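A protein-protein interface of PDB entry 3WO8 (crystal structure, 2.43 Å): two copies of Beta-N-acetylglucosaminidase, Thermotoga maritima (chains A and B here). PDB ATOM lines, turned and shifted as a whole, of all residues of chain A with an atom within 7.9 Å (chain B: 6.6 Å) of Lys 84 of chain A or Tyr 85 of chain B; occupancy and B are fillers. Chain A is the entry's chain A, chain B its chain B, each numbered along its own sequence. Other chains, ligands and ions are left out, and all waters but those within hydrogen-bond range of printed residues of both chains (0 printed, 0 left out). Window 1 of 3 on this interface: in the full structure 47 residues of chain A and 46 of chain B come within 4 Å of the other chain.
N of Ser 88 of chain B is in hydrogen-bond range of OE2 of Glu 53 of chain A (3.2 Å).
N of Ser 88 of chain A lies within hydrogen-bond range of OE2 of Glu 53 of chain B (3.0 Å).
The backbone carbonyl oxygen (O) of Lys 84 of chain A is in hydrogen-bond range of the side-chain amino group (NZ) of Lys 84 of chain B.
The side-chain carboxylate of Glu 81 of chain A lies within hydrogen-bond range of the side-chain hydroxyl of Ser 88 of chain A.
The side-chain carboxylate (OE1) of Glu 53 of chain B lies within salt-bridge range of the side-chain amino group (NZ) of Lys 84 of chain B (3.3 Å).
NZ of Lys 84 of chain A lies within salt-bridge range of OE1 of Glu 53 of chain A (3.1 Å).
O of Val 117 of chain B lies within hydrogen-bond range of N of Val 333 of chain B (2.9 Å).
OE1 of Glu 81 of chain B sits at hydrogen-bond distance from OG of Ser 88 of chain B, at 2.7 Å.
OH of Tyr 85 of chain A sits at hydrogen-bond distance from OE2 of Glu 53 of chain A, at 2.4 Å.
Among the printed residues, pairs that only touch across the chains: Glu 53 of chain A with Pro 87 of chain B, Met 57 of chain A with Ser 88 of chain B, Lys 84 of chain A with Tyr 85 of chain B, Tyr 85 of chain A with Lys 84 of chain B, Tyr 85 of chain A with Tyr 85 of chain B, Tyr 85 of chain A with Pro 87 of chain B, Pro 87 of chain A with Glu 53 of chain B, Pro 87 of chain A with Tyr 85 of chain B, Pro 87 of chain A with Val 333 of chain B and Ser 88 of chain A with Met 57 of chain B.
Of the printed residues of chain B, Glu 53 of chain A touches Pro 87 and Ser 88.
Lys 84 of chain A touches just these residues of chain B: Lys 84 and Tyr 85.
Printed residues of chain B within 4 Å of Tyr 85 of chain A: Lys 84, Tyr 85 and Pro 87.
Of the printed residues of chain B, Pro 87 of chain A touches Glu 53 (3.3 Å), Tyr 85 (3.7 Å) and Val 333 (3.4 Å).
Of the printed residues of chain A, Met 57 of chain B touches Ser 88.
Tyr 85 of chain B touches three residues of chain A.
Val 86 of chain B touches none of the printed residues of chain A.
The nearest residue of chain B that does not touch Lys 84 of chain A is Val 86 of chain B (4.3 Å).
The nearest residue of chain A that does not touch Tyr 85 of chain B is Val 86 of chain A (4.3 Å).
Of the 18 printed residues of chain B, 7 touch a printed residue of chain A.
Hydrophobic or aromatic side chains of chain B within 4 Å of the printed part of chain A: Met 57, Tyr 85, Pro 87 and Val 333.
Hydrophobic or aromatic side chains of chain A within 4 Å of the printed part of chain B: Met 57, Tyr 85 and Pro 87.
Along chain A the printed residues that touch a printed residue of chain B span positions 53 to 88.
Among the printed residues, 13 pairs touch across the chains.
Among the printed residues, no Asp or Glu carboxylate lies within 4 Å of a Lys or Arg side-chain nitrogen of the other chain.
Glu 53 of chain A touches Ser 88 of chain B, and with the chains exchanged Ser 88 of chain A touches Glu 53 of chain B.
Lys 84 of chain B touches its own counterpart, Lys 84 of chain A.
Lys 84 of chain A touches Tyr 85 of chain B, and with the chains exchanged Tyr 85 of chain A touches Lys 84 of chain B.
Tyr 85 of chain A touches Pro 87 of chain B, and with the chains exchanged Pro 87 of chain A touches Tyr 85 of chain B.
Of the 13 pairs that touch across the chains among the printed residues, 12 have their exchanged pair printed and touching as well.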
ATOM      1  N   LEU A  50     -20.304 -16.019 -16.944  1.00  0.00           N
ATOM      2  CA  LEU A  50     -20.778 -15.936 -15.551  1.00  0.00           C
ATOM      3  C   LEU A  50     -22.140 -16.590 -15.307  1.00  0.00           C
ATOM      4  O   LEU A  50     -22.340 -17.212 -14.281  1.00  0.00           O
ATOM      5  CB  LEU A  50     -20.833 -14.480 -15.115  1.00  0.00           C
ATOM      6  CG  LEU A  50     -19.517 -13.725 -15.111  1.00  0.00           C
ATOM      7  CD1 LEU A  50     -19.753 -12.228 -14.931  1.00  0.00           C
ATOM      8  CD2 LEU A  50     -18.663 -14.267 -13.973  1.00  0.00           C
ATOM      9  N   SER A  51     -23.048 -16.458 -16.271  1.00  0.00           N
ATOM     10  CA  SER A  51     -24.400 -17.044 -16.219  1.00  0.00           C
ATOM     11  C   SER A  51     -24.399 -18.539 -16.373  1.00  0.00           C
ATOM     12  O   SER A  51     -25.451 -19.157 -16.416  1.00  0.00           O
ATOM     13  CB  SER A  51     -25.233 -16.491 -17.376  1.00  0.00           C
ATOM     14  OG  SER A  51     -24.657 -16.926 -18.611  1.00  0.00           O
ATOM     15  N   LYS A  52     -23.231 -19.123 -16.544  1.00  0.00           N
ATOM     16  CA  LYS A  52     -23.102 -20.556 -16.673  1.00  0.00           C
ATOM     17  C   LYS A  52     -21.991 -20.973 -15.718  1.00  0.00           C
ATOM     18  O   LYS A  52     -20.802 -21.076 -16.054  1.00  0.00           O
ATOM     19  CB  LYS A  52     -22.820 -20.944 -18.104  1.00  0.00           C
ATOM     20  CG  LYS A  52     -24.064 -21.410 -18.780  1.00  0.00           C
ATOM     21  CD  LYS A  52     -23.965 -21.386 -20.292  1.00  0.00           C
ATOM     22  CE  LYS A  52     -25.346 -21.515 -20.923  1.00  0.00           C
ATOM     23  NZ  LYS A  52     -26.335 -20.489 -20.451  1.00  0.00           N
ATOM     24  N   GLU A  53     -22.420 -21.215 -14.501  1.00  0.00           N
ATOM     25  CA  GLU A  53     -21.537 -21.346 -13.391  1.00  0.00           C
ATOM     26  C   GLU A  53     -20.548 -22.518 -13.607  1.00  0.00           C
ATOM     27  O   GLU A  53     -19.436 -22.493 -13.137  1.00  0.00           O
ATOM     28  CB  GLU A  53     -22.404 -21.460 -12.148  1.00  0.00           C
ATOM     29  CG  GLU A  53     -21.695 -21.592 -10.834  1.00  0.00           C
ATOM     30  CD  GLU A  53     -22.645 -21.415  -9.659  1.00  0.00           C
ATOM     31  OE1 GLU A  53     -23.697 -22.063  -9.650  1.00  0.00           O
ATOM     32  OE2 GLU A  53     -22.354 -20.640  -8.743  1.00  0.00           O
ATOM     33  N   LEU A  56     -17.777 -20.807 -15.600  1.00  0.00           N
ATOM     34  CA  LEU A  56     -17.027 -19.965 -14.719  1.00  0.00           C
ATOM     35  C   LEU A  56     -16.035 -20.803 -13.851  1.00  0.00           C
ATOM     36  O   LEU A  56     -14.865 -20.460 -13.700  1.00  0.00           O
ATOM     37  CB  LEU A  56     -17.977 -19.184 -13.838  1.00  0.00           C
ATOM     38  CG  LEU A  56     -17.339 -18.423 -12.677  1.00  0.00           C
ATOM     39  CD1 LEU A  56     -16.280 -17.469 -13.143  1.00  0.00           C
ATOM     40  CD2 LEU A  56     -18.409 -17.639 -11.940  1.00  0.00           C
ATOM     41  N   MET A  57     -16.510 -21.900 -13.299  1.00  0.00           N
ATOM     42  CA  MET A  57     -15.709 -22.694 -12.407  1.00  0.00           C
ATOM     43  C   MET A  57     -14.528 -23.288 -13.156  1.00  0.00           C
ATOM     44  O   MET A  57     -13.433 -23.229 -12.679  1.00  0.00           O
ATOM     45  CB  MET A  57     -16.545 -23.797 -11.759  1.00  0.00           C
ATOM     46  CG  MET A  57     -17.488 -23.325 -10.644  1.00  0.00           C
ATOM     47  SD  MET A  57     -18.727 -24.579 -10.160  1.00  0.00           S
ATOM     48  CE  MET A  57     -19.562 -23.673  -8.857  1.00  0.00           C
ATOM     49  N   HIS A  75     -19.045  -5.556 -12.380  1.00  0.00           N
ATOM     50  CA  HIS A  75     -20.118  -5.582 -11.428  1.00  0.00           C
ATOM     51  C   HIS A  75     -20.112  -4.349 -10.548  1.00  0.00           C
ATOM     52  O   HIS A  75     -19.663  -4.377  -9.442  1.00  0.00           O
ATOM     53  CB  HIS A  75     -20.051  -6.829 -10.596  1.00  0.00           C
ATOM     54  CG  HIS A  75     -21.331  -7.114  -9.911  1.00  0.00           C
ATOM     55  ND1 HIS A  75     -21.758  -6.419  -8.806  1.00  0.00           N
ATOM     56  CD2 HIS A  75     -22.334  -7.950 -10.226  1.00  0.00           C
ATOM     57  CE1 HIS A  75     -22.943  -6.860  -8.433  1.00  0.00           C
ATOM     58  NE2 HIS A  75     -23.326  -7.775  -9.290  1.00  0.00           N
ATOM     59  N   GLU A  81     -25.064  -5.205 -13.353  1.00  0.00           N
ATOM     60  CA  GLU A  81     -24.826  -6.314 -12.412  1.00  0.00           C
ATOM     61  C   GLU A  81     -24.748  -7.589 -13.207  1.00  0.00           C
ATOM     62  O   GLU A  81     -25.584  -7.816 -14.068  1.00  0.00           O
ATOM     63  CB  GLU A  81     -25.950  -6.411 -11.399  1.00  0.00           C
ATOM     64  CG  GLU A  81     -25.954  -5.249 -10.418  1.00  0.00           C
ATOM     65  CD  GLU A  81     -27.032  -5.312  -9.351  1.00  0.00           C
ATOM     66  OE1 GLU A  81     -28.018  -6.028  -9.498  1.00  0.00           O
ATOM     67  OE2 GLU A  81     -26.874  -4.620  -8.351  1.00  0.00           O
ATOM     68  N   VAL A  82     -23.696  -8.368 -12.972  1.00  0.00           N
ATOM     69  CA  VAL A  82     -23.421  -9.591 -13.725  1.00  0.00           C
ATOM     70  C   VAL A  82     -23.093 -10.807 -12.836  1.00  0.00           C
ATOM     71  O   VAL A  82     -23.048 -11.933 -13.298  1.00  0.00           O
ATOM     72  CB  VAL A  82     -22.252  -9.346 -14.711  1.00  0.00           C
ATOM     73  CG1 VAL A  82     -22.582  -8.186 -15.664  1.00  0.00           C
ATOM     74  CG2 VAL A  82     -20.965  -9.050 -13.956  1.00  0.00           C
ATOM     75  N   LEU A  83     -22.873 -10.560 -11.564  1.00  0.00           N
ATOM     76  CA  LEU A  83     -22.484 -11.578 -10.609  1.00  0.00           C
ATOM     77  C   LEU A  83     -23.684 -11.926  -9.798  1.00  0.00           C
ATOM     78  O   LEU A  83     -24.177 -11.110  -9.039  1.00  0.00           O
ATOM     79  CB  LEU A  83     -21.404 -11.069  -9.655  1.00  0.00           C
ATOM     80  CG  LEU A  83     -19.992 -10.997 -10.242  1.00  0.00           C
ATOM     81  CD1 LEU A  83     -19.081 -10.221  -9.312  1.00  0.00           C
ATOM     82  CD2 LEU A  83     -19.481 -12.420 -10.467  1.00  0.00           C
ATOM     83  N   LYS A  84     -24.151 -13.144  -9.958  1.00  0.00           N
ATOM     84  CA  LYS A  84     -25.300 -13.587  -9.200  1.00  0.00           C
ATOM     85  C   LYS A  84     -25.019 -13.588  -7.696  1.00  0.00           C
ATOM     86  O   LYS A  84     -25.865 -13.185  -6.916  1.00  0.00           O
ATOM     87  CB  LYS A  84     -25.818 -14.941  -9.698  1.00  0.00           C
ATOM     88  CG  LYS A  84     -24.959 -16.166  -9.452  1.00  0.00           C
ATOM     89  CD  LYS A  84     -25.872 -17.401  -9.438  1.00  0.00           C
ATOM     90  CE  LYS A  84     -25.068 -18.691  -9.493  1.00  0.00           C
ATOM     91  NZ  LYS A  84     -25.690 -19.830  -8.742  1.00  0.00           N
ATOM     92  N   TYR A  85     -23.791 -13.939  -7.339  1.00  0.00           N
ATOM     93  CA  TYR A  85     -23.326 -14.044  -5.943  1.00  0.00           C
ATOM     94  C   TYR A  85     -23.427 -12.800  -5.110  1.00  0.00           C
ATOM     95  O   TYR A  85     -23.399 -12.862  -3.911  1.00  0.00           O
ATOM     96  CB  TYR A  85     -21.872 -14.464  -5.920  1.00  0.00           C
ATOM     97  CG  TYR A  85     -21.617 -15.609  -6.829  1.00  0.00           C
ATOM     98  CD1 TYR A  85     -22.166 -16.828  -6.562  1.00  0.00           C
ATOM     99  CD2 TYR A  85     -20.877 -15.450  -7.990  1.00  0.00           C
ATOM    100  CE1 TYR A  85     -21.965 -17.885  -7.411  1.00  0.00           C
ATOM    101  CE2 TYR A  85     -20.644 -16.488  -8.823  1.00  0.00           C
ATOM    102  CZ  TYR A  85     -21.182 -17.710  -8.542  1.00  0.00           C
ATOM    103  OH  TYR A  85     -20.966 -18.771  -9.409  1.00  0.00           O
ATOM    104  N   VAL A  86     -23.553 -11.660  -5.730  1.00  0.00           N
ATOM    105  CA  VAL A  86     -23.471 -10.434  -4.982  1.00  0.00           C
ATOM    106  C   VAL A  86     -24.823  -9.793  -4.838  1.00  0.00           C
ATOM    107  O   VAL A  86     -25.438  -9.441  -5.839  1.00  0.00           O
ATOM    108  CB  VAL A  86     -22.554  -9.433  -5.708  1.00  0.00           C
ATOM    109  CG1 VAL A  86     -22.678  -8.018  -5.166  1.00  0.00           C
ATOM    110  CG2 VAL A  86     -21.134  -9.935  -5.623  1.00  0.00           C
ATOM    111  N   PRO A  87     -25.254  -9.552  -3.595  1.00  0.00           N
ATOM    112  CA  PRO A  87     -26.555  -8.915  -3.379  1.00  0.00           C
ATOM    113  C   PRO A  87     -26.752  -7.683  -4.239  1.00  0.00           C
ATOM    114  O   PRO A  87     -25.865  -6.874  -4.391  1.00  0.00           O
ATOM    115  CB  PRO A  87     -26.495  -8.522  -1.911  1.00  0.00           C
ATOM    116  CG  PRO A  87     -25.661  -9.608  -1.303  1.00  0.00           C
ATOM    117  CD  PRO A  87     -24.563  -9.793  -2.315  1.00  0.00           C
ATOM    118  N   SER A  88     -27.917  -7.594  -4.816  1.00  0.00           N
ATOM    119  CA  SER A  88     -28.248  -6.510  -5.670  1.00  0.00           C
ATOM    120  C   SER A  88     -28.254  -5.192  -4.959  1.00  0.00           C
ATOM    121  O   SER A  88     -28.650  -5.061  -3.837  1.00  0.00           O
ATOM    122  CB  SER A  88     -29.599  -6.719  -6.362  1.00  0.00           C
ATOM    123  OG  SER A  88     -29.859  -5.593  -7.191  1.00  0.00           O
ATOM    124  N   ILE A 113     -17.238 -10.990  -1.546  1.00  0.00           N
ATOM    125  CA  ILE A 113     -17.863 -12.096  -2.293  1.00  0.00           C
ATOM    126  C   ILE A 113     -17.076 -12.334  -3.567  1.00  0.00           C
ATOM    127  O   ILE A 113     -16.840 -13.466  -3.935  1.00  0.00           O
ATOM    128  CB  ILE A 113     -19.361 -11.856  -2.622  1.00  0.00           C
ATOM    129  CG1 ILE A 113     -20.176 -11.930  -1.334  1.00  0.00           C
ATOM    130  CG2 ILE A 113     -19.874 -12.905  -3.623  1.00  0.00           C
ATOM    131  CD1 ILE A 113     -21.533 -11.264  -1.400  1.00  0.00           C
ATOM    132  N   ILE A 116     -14.044 -14.460  -2.817  1.00  0.00           N
ATOM    133  CA  ILE A 116     -14.361 -15.854  -2.624  1.00  0.00           C
ATOM    134  C   ILE A 116     -14.567 -16.545  -3.968  1.00  0.00           C
ATOM    135  O   ILE A 116     -14.145 -17.663  -4.213  1.00  0.00           O
ATOM    136  CB  ILE A 116     -15.651 -15.976  -1.812  1.00  0.00           C
ATOM    137  CG1 ILE A 116     -15.392 -15.535  -0.374  1.00  0.00           C
ATOM    138  CG2 ILE A 116     -16.192 -17.394  -1.880  1.00  0.00           C
ATOM    139  CD1 ILE A 116     -16.650 -15.246   0.397  1.00  0.00           C
ATOM    140  N   VAL A 117     -15.272 -15.866  -4.828  1.00  0.00           N
ATOM    141  CA  VAL A 117     -15.539 -16.364  -6.133  1.00  0.00           C
ATOM    142  C   VAL A 117     -14.266 -16.515  -6.942  1.00  0.00           C
ATOM    143  O   VAL A 117     -14.193 -17.398  -7.768  1.00  0.00           O
ATOM    144  CB  VAL A 117     -16.453 -15.366  -6.843  1.00  0.00           C
ATOM    145  CG1 VAL A 117     -16.428 -15.578  -8.340  1.00  0.00           C
ATOM    146  CG2 VAL A 117     -17.842 -15.510  -6.278  1.00  0.00           C
ATOM    147  N   LEU B  50     -36.515 -16.070  -1.077  1.00  0.00           N
ATOM    148  CA  LEU B  50     -35.132 -16.033  -1.599  1.00  0.00           C
ATOM    149  C   LEU B  50     -35.109 -15.644  -3.048  1.00  0.00           C
ATOM    150  O   LEU B  50     -34.399 -14.753  -3.463  1.00  0.00           O
ATOM    151  CB  LEU B  50     -34.403 -17.357  -1.422  1.00  0.00           C
ATOM    152  CG  LEU B  50     -34.389 -17.880   0.031  1.00  0.00           C
ATOM    153  CD1 LEU B  50     -33.753 -19.277   0.197  1.00  0.00           C
ATOM    154  CD2 LEU B  50     -33.708 -16.867   0.938  1.00  0.00           C
ATOM    155  N   GLU B  53     -35.289 -11.168  -4.515  1.00  0.00           N
ATOM    156  CA  GLU B  53     -34.338 -10.545  -3.647  1.00  0.00           C
ATOM    157  C   GLU B  53     -34.904  -9.323  -2.886  1.00  0.00           C
ATOM    158  O   GLU B  53     -34.669  -9.200  -1.689  1.00  0.00           O
ATOM    159  CB  GLU B  53     -33.102 -10.234  -4.450  1.00  0.00           C
ATOM    160  CG  GLU B  53     -32.035  -9.496  -3.733  1.00  0.00           C
ATOM    161  CD  GLU B  53     -30.743  -9.576  -4.498  1.00  0.00           C
ATOM    162  OE1 GLU B  53     -30.752  -9.403  -5.728  1.00  0.00           O
ATOM    163  OE2 GLU B  53     -29.724  -9.863  -3.874  1.00  0.00           O
ATOM    164  N   LEU B  56     -36.538 -10.623   0.114  1.00  0.00           N
ATOM    165  CA  LEU B  56     -35.518 -11.078   1.029  1.00  0.00           C
ATOM    166  C   LEU B  56     -34.936  -9.910   1.793  1.00  0.00           C
ATOM    167  O   LEU B  56     -34.746  -9.985   2.990  1.00  0.00           O
ATOM    168  CB  LEU B  56     -34.392 -11.810   0.304  1.00  0.00           C
ATOM    169  CG  LEU B  56     -33.325 -12.250   1.292  1.00  0.00           C
ATOM    170  CD1 LEU B  56     -33.925 -13.149   2.382  1.00  0.00           C
ATOM    171  CD2 LEU B  56     -32.203 -12.927   0.576  1.00  0.00           C
ATOM    172  N   MET B  57     -34.686  -8.815   1.092  1.00  0.00           N
ATOM    173  CA  MET B  57     -34.146  -7.640   1.746  1.00  0.00           C
ATOM    174  C   MET B  57     -35.103  -7.016   2.753  1.00  0.00           C
ATOM    175  O   MET B  57     -34.722  -6.673   3.864  1.00  0.00           O
ATOM    176  CB  MET B  57     -33.691  -6.602   0.711  1.00  0.00           C
ATOM    177  CG  MET B  57     -32.445  -7.018  -0.082  1.00  0.00           C
ATOM    178  SD  MET B  57     -32.184  -6.011  -1.559  1.00  0.00           S
ATOM    179  CE  MET B  57     -30.673  -6.835  -2.091  1.00  0.00           C
ATOM    180  N   HIS B  75     -30.151 -24.566   2.442  1.00  0.00           N
ATOM    181  CA  HIS B  75     -29.112 -24.605   1.445  1.00  0.00           C
ATOM    182  C   HIS B  75     -28.052 -25.629   1.813  1.00  0.00           C
ATOM    183  O   HIS B  75     -27.029 -25.293   2.381  1.00  0.00           O
ATOM    184  CB  HIS B  75     -28.480 -23.234   1.298  1.00  0.00           C
ATOM    185  CG  HIS B  75     -27.897 -23.021  -0.039  1.00  0.00           C
ATOM    186  ND1 HIS B  75     -26.644 -23.467  -0.397  1.00  0.00           N
ATOM    187  CD2 HIS B  75     -28.432 -22.468  -1.139  1.00  0.00           C
ATOM    188  CE1 HIS B  75     -26.417 -23.152  -1.660  1.00  0.00           C
ATOM    189  NE2 HIS B  75     -27.494 -22.554  -2.135  1.00  0.00           N
ATOM    190  N   GLU B  81     -30.572 -26.585  -3.233  1.00  0.00           N
ATOM    191  CA  GLU B  81     -29.898 -25.280  -3.269  1.00  0.00           C
ATOM    192  C   GLU B  81     -30.948 -24.217  -3.460  1.00  0.00           C
ATOM    193  O   GLU B  81     -31.786 -24.359  -4.287  1.00  0.00           O
ATOM    194  CB  GLU B  81     -28.839 -25.207  -4.384  1.00  0.00           C
ATOM    195  CG  GLU B  81     -27.646 -26.105  -4.144  1.00  0.00           C
ATOM    196  CD  GLU B  81     -26.492 -25.944  -5.158  1.00  0.00           C
ATOM    197  OE1 GLU B  81     -26.743 -25.570  -6.328  1.00  0.00           O
ATOM    198  OE2 GLU B  81     -25.320 -26.192  -4.767  1.00  0.00           O
ATOM    199  N   VAL B  82     -30.895 -23.181  -2.650  1.00  0.00           N
ATOM    200  CA  VAL B  82     -31.928 -22.160  -2.579  1.00  0.00           C
ATOM    201  C   VAL B  82     -31.398 -20.722  -2.541  1.00  0.00           C
ATOM    202  O   VAL B  82     -32.167 -19.773  -2.691  1.00  0.00           O
ATOM    203  CB  VAL B  82     -32.845 -22.380  -1.322  1.00  0.00           C
ATOM    204  CG1 VAL B  82     -33.517 -23.742  -1.375  1.00  0.00           C
ATOM    205  CG2 VAL B  82     -32.084 -22.275   0.000  1.00  0.00           C
ATOM    206  N   LEU B  83     -30.103 -20.539  -2.343  1.00  0.00           N
ATOM    207  CA  LEU B  83     -29.513 -19.219  -2.217  1.00  0.00           C
ATOM    208  C   LEU B  83     -28.711 -18.934  -3.474  1.00  0.00           C
ATOM    209  O   LEU B  83     -27.748 -19.651  -3.777  1.00  0.00           O
ATOM    210  CB  LEU B  83     -28.564 -19.154  -1.046  1.00  0.00           C
ATOM    211  CG  LEU B  83     -29.102 -19.405   0.364  1.00  0.00           C
ATOM    212  CD1 LEU B  83     -27.950 -19.615   1.355  1.00  0.00           C
ATOM    213  CD2 LEU B  83     -29.935 -18.223   0.821  1.00  0.00           C
ATOM    214  N   LYS B  84     -29.098 -17.901  -4.218  1.00  0.00           N
ATOM    215  CA  LYS B  84     -28.367 -17.549  -5.435  1.00  0.00           C
ATOM    216  C   LYS B  84     -26.920 -17.159  -5.159  1.00  0.00           C
ATOM    217  O   LYS B  84     -26.049 -17.434  -5.966  1.00  0.00           O
ATOM    218  CB  LYS B  84     -29.061 -16.427  -6.210  1.00  0.00           C
ATOM    219  CG  LYS B  84     -29.140 -15.069  -5.542  1.00  0.00           C
ATOM    220  CD  LYS B  84     -30.159 -14.170  -6.268  1.00  0.00           C
ATOM    221  CE  LYS B  84     -29.574 -13.297  -7.380  1.00  0.00           C
ATOM    222  NZ  LYS B  84     -29.099 -11.988  -6.801  1.00  0.00           N
ATOM    223  N   TYR B  85     -26.684 -16.596  -3.978  1.00  0.00           N
ATOM    224  CA  TYR B  85     -25.406 -16.065  -3.564  1.00  0.00           C
ATOM    225  C   TYR B  85     -24.281 -17.080  -3.357  1.00  0.00           C
ATOM    226  O   TYR B  85     -23.119 -16.724  -3.334  1.00  0.00           O
ATOM    227  CB  TYR B  85     -25.585 -15.303  -2.264  1.00  0.00           C
ATOM    228  CG  TYR B  85     -26.762 -14.372  -2.285  1.00  0.00           C
ATOM    229  CD1 TYR B  85     -26.756 -13.262  -3.102  1.00  0.00           C
ATOM    230  CD2 TYR B  85     -27.890 -14.605  -1.490  1.00  0.00           C
ATOM    231  CE1 TYR B  85     -27.806 -12.387  -3.128  1.00  0.00           C
ATOM    232  CE2 TYR B  85     -28.974 -13.735  -1.507  1.00  0.00           C
ATOM    233  CZ  TYR B  85     -28.920 -12.619  -2.336  1.00  0.00           C
ATOM    234  OH  TYR B  85     -29.953 -11.723  -2.395  1.00  0.00           O
ATOM    235  N   VAL B  86     -24.611 -18.336  -3.181  1.00  0.00           N
ATOM    236  CA  VAL B  86     -23.608 -19.304  -2.836  1.00  0.00           C
ATOM    237  C   VAL B  86     -23.256 -20.051  -4.073  1.00  0.00           C
ATOM    238  O   VAL B  86     -24.133 -20.457  -4.813  1.00  0.00           O
ATOM    239  CB  VAL B  86     -24.115 -20.267  -1.737  1.00  0.00           C
ATOM    240  CG1 VAL B  86     -23.105 -21.365  -1.419  1.00  0.00           C
ATOM    241  CG2 VAL B  86     -24.399 -19.473  -0.477  1.00  0.00           C
ATOM    242  N   PRO B  87     -21.960 -20.210  -4.326  1.00  0.00           N
ATOM    243  CA  PRO B  87     -21.603 -21.003  -5.462  1.00  0.00           C
ATOM    244  C   PRO B  87     -22.198 -22.348  -5.322  1.00  0.00           C
ATOM    245  O   PRO B  87     -22.172 -22.925  -4.261  1.00  0.00           O
ATOM    246  CB  PRO B  87     -20.097 -21.089  -5.358  1.00  0.00           C
ATOM    247  CG  PRO B  87     -19.717 -19.765  -4.786  1.00  0.00           C
ATOM    248  CD  PRO B  87     -20.827 -19.424  -3.816  1.00  0.00           C
ATOM    249  N   SER B  88     -22.749 -22.851  -6.397  1.00  0.00           N
ATOM    250  CA  SER B  88     -23.281 -24.175  -6.432  1.00  0.00           C
ATOM    251  C   SER B  88     -22.187 -25.181  -6.169  1.00  0.00           C
ATOM    252  O   SER B  88     -21.028 -24.890  -6.336  1.00  0.00           O
ATOM    253  CB  SER B  88     -24.006 -24.448  -7.755  1.00  0.00           C
ATOM    254  OG  SER B  88     -24.474 -25.792  -7.829  1.00  0.00           O
ATOM    255  N   ILE B 113     -20.749 -16.431   3.080  1.00  0.00           N
ATOM    256  CA  ILE B 113     -21.793 -15.798   2.292  1.00  0.00           C
ATOM    257  C   ILE B 113     -23.174 -15.735   2.996  1.00  0.00           C
ATOM    258  O   ILE B 113     -23.872 -14.731   2.947  1.00  0.00           O
ATOM    259  CB  ILE B 113     -21.873 -16.467   0.911  1.00  0.00           C
ATOM    260  CG1 ILE B 113     -20.569 -16.144   0.137  1.00  0.00           C
ATOM    261  CG2 ILE B 113     -23.078 -15.935   0.144  1.00  0.00           C
ATOM    262  CD1 ILE B 113     -20.412 -16.971  -1.129  1.00  0.00           C
ATOM    263  N   MET B 114     -23.572 -16.807   3.644  1.00  0.00           N
ATOM    264  CA  MET B 114     -24.839 -16.784   4.338  1.00  0.00           C
ATOM    265  C   MET B 114     -24.817 -15.635   5.313  1.00  0.00           C
ATOM    266  O   MET B 114     -25.780 -14.874   5.467  1.00  0.00           O
ATOM    267  CB  MET B 114     -25.055 -18.109   5.067  1.00  0.00           C
ATOM    268  CG  MET B 114     -25.611 -19.200   4.177  1.00  0.00           C
ATOM    269  SD  MET B 114     -25.242 -20.804   4.882  1.00  0.00           S
ATOM    270  CE  MET B 114     -25.487 -21.915   3.498  1.00  0.00           C
ATOM    271  N   VAL B 117     -25.292 -12.228   3.913  1.00  0.00           N
ATOM    272  CA  VAL B 117     -26.651 -12.107   3.433  1.00  0.00           C
ATOM    273  C   VAL B 117     -27.566 -11.854   4.625  1.00  0.00           C
ATOM    274  O   VAL B 117     -28.556 -11.138   4.526  1.00  0.00           O
ATOM    275  CB  VAL B 117     -27.060 -13.421   2.761  1.00  0.00           C
ATOM    276  CG1 VAL B 117     -28.518 -13.412   2.413  1.00  0.00           C
ATOM    277  CG2 VAL B 117     -26.265 -13.679   1.500  1.00  0.00           C
ATOM    278  N   LEU B 119     -28.194 -14.640   7.072  1.00  0.00           N
ATOM    279  CA  LEU B 119     -28.477 -15.882   7.715  1.00  0.00           C
ATOM    280  C   LEU B 119     -27.454 -16.120   8.825  1.00  0.00           C
ATOM    281  O   LEU B 119     -26.271 -15.768   8.700  1.00  0.00           O
ATOM    282  CB  LEU B 119     -28.364 -17.031   6.721  1.00  0.00           C
ATOM    283  CG  LEU B 119     -29.393 -17.257   5.617  1.00  0.00           C
ATOM    284  CD1 LEU B 119     -30.788 -16.822   6.041  1.00  0.00           C
ATOM    285  CD2 LEU B 119     -28.952 -16.558   4.346  1.00  0.00           C
ATOM    286  N   VAL B 333     -28.293  -8.230   4.280  1.00  0.00           N
ATOM    287  CA  VAL B 333     -28.812  -7.635   3.068  1.00  0.00           C
ATOM    288  C   VAL B 333     -29.927  -6.565   3.350  1.00  0.00           C
ATOM    289  O   VAL B 333     -30.192  -5.631   2.561  1.00  0.00           O
ATOM    290  CB  VAL B 333     -29.183  -8.845   2.189  1.00  0.00           C
ATOM    291  CG1 VAL B 333     -30.654  -9.080   2.135  1.00  0.00           C
ATOM    292  CG2 VAL B 333     -28.541  -8.734   0.837  1.00  0.00           C
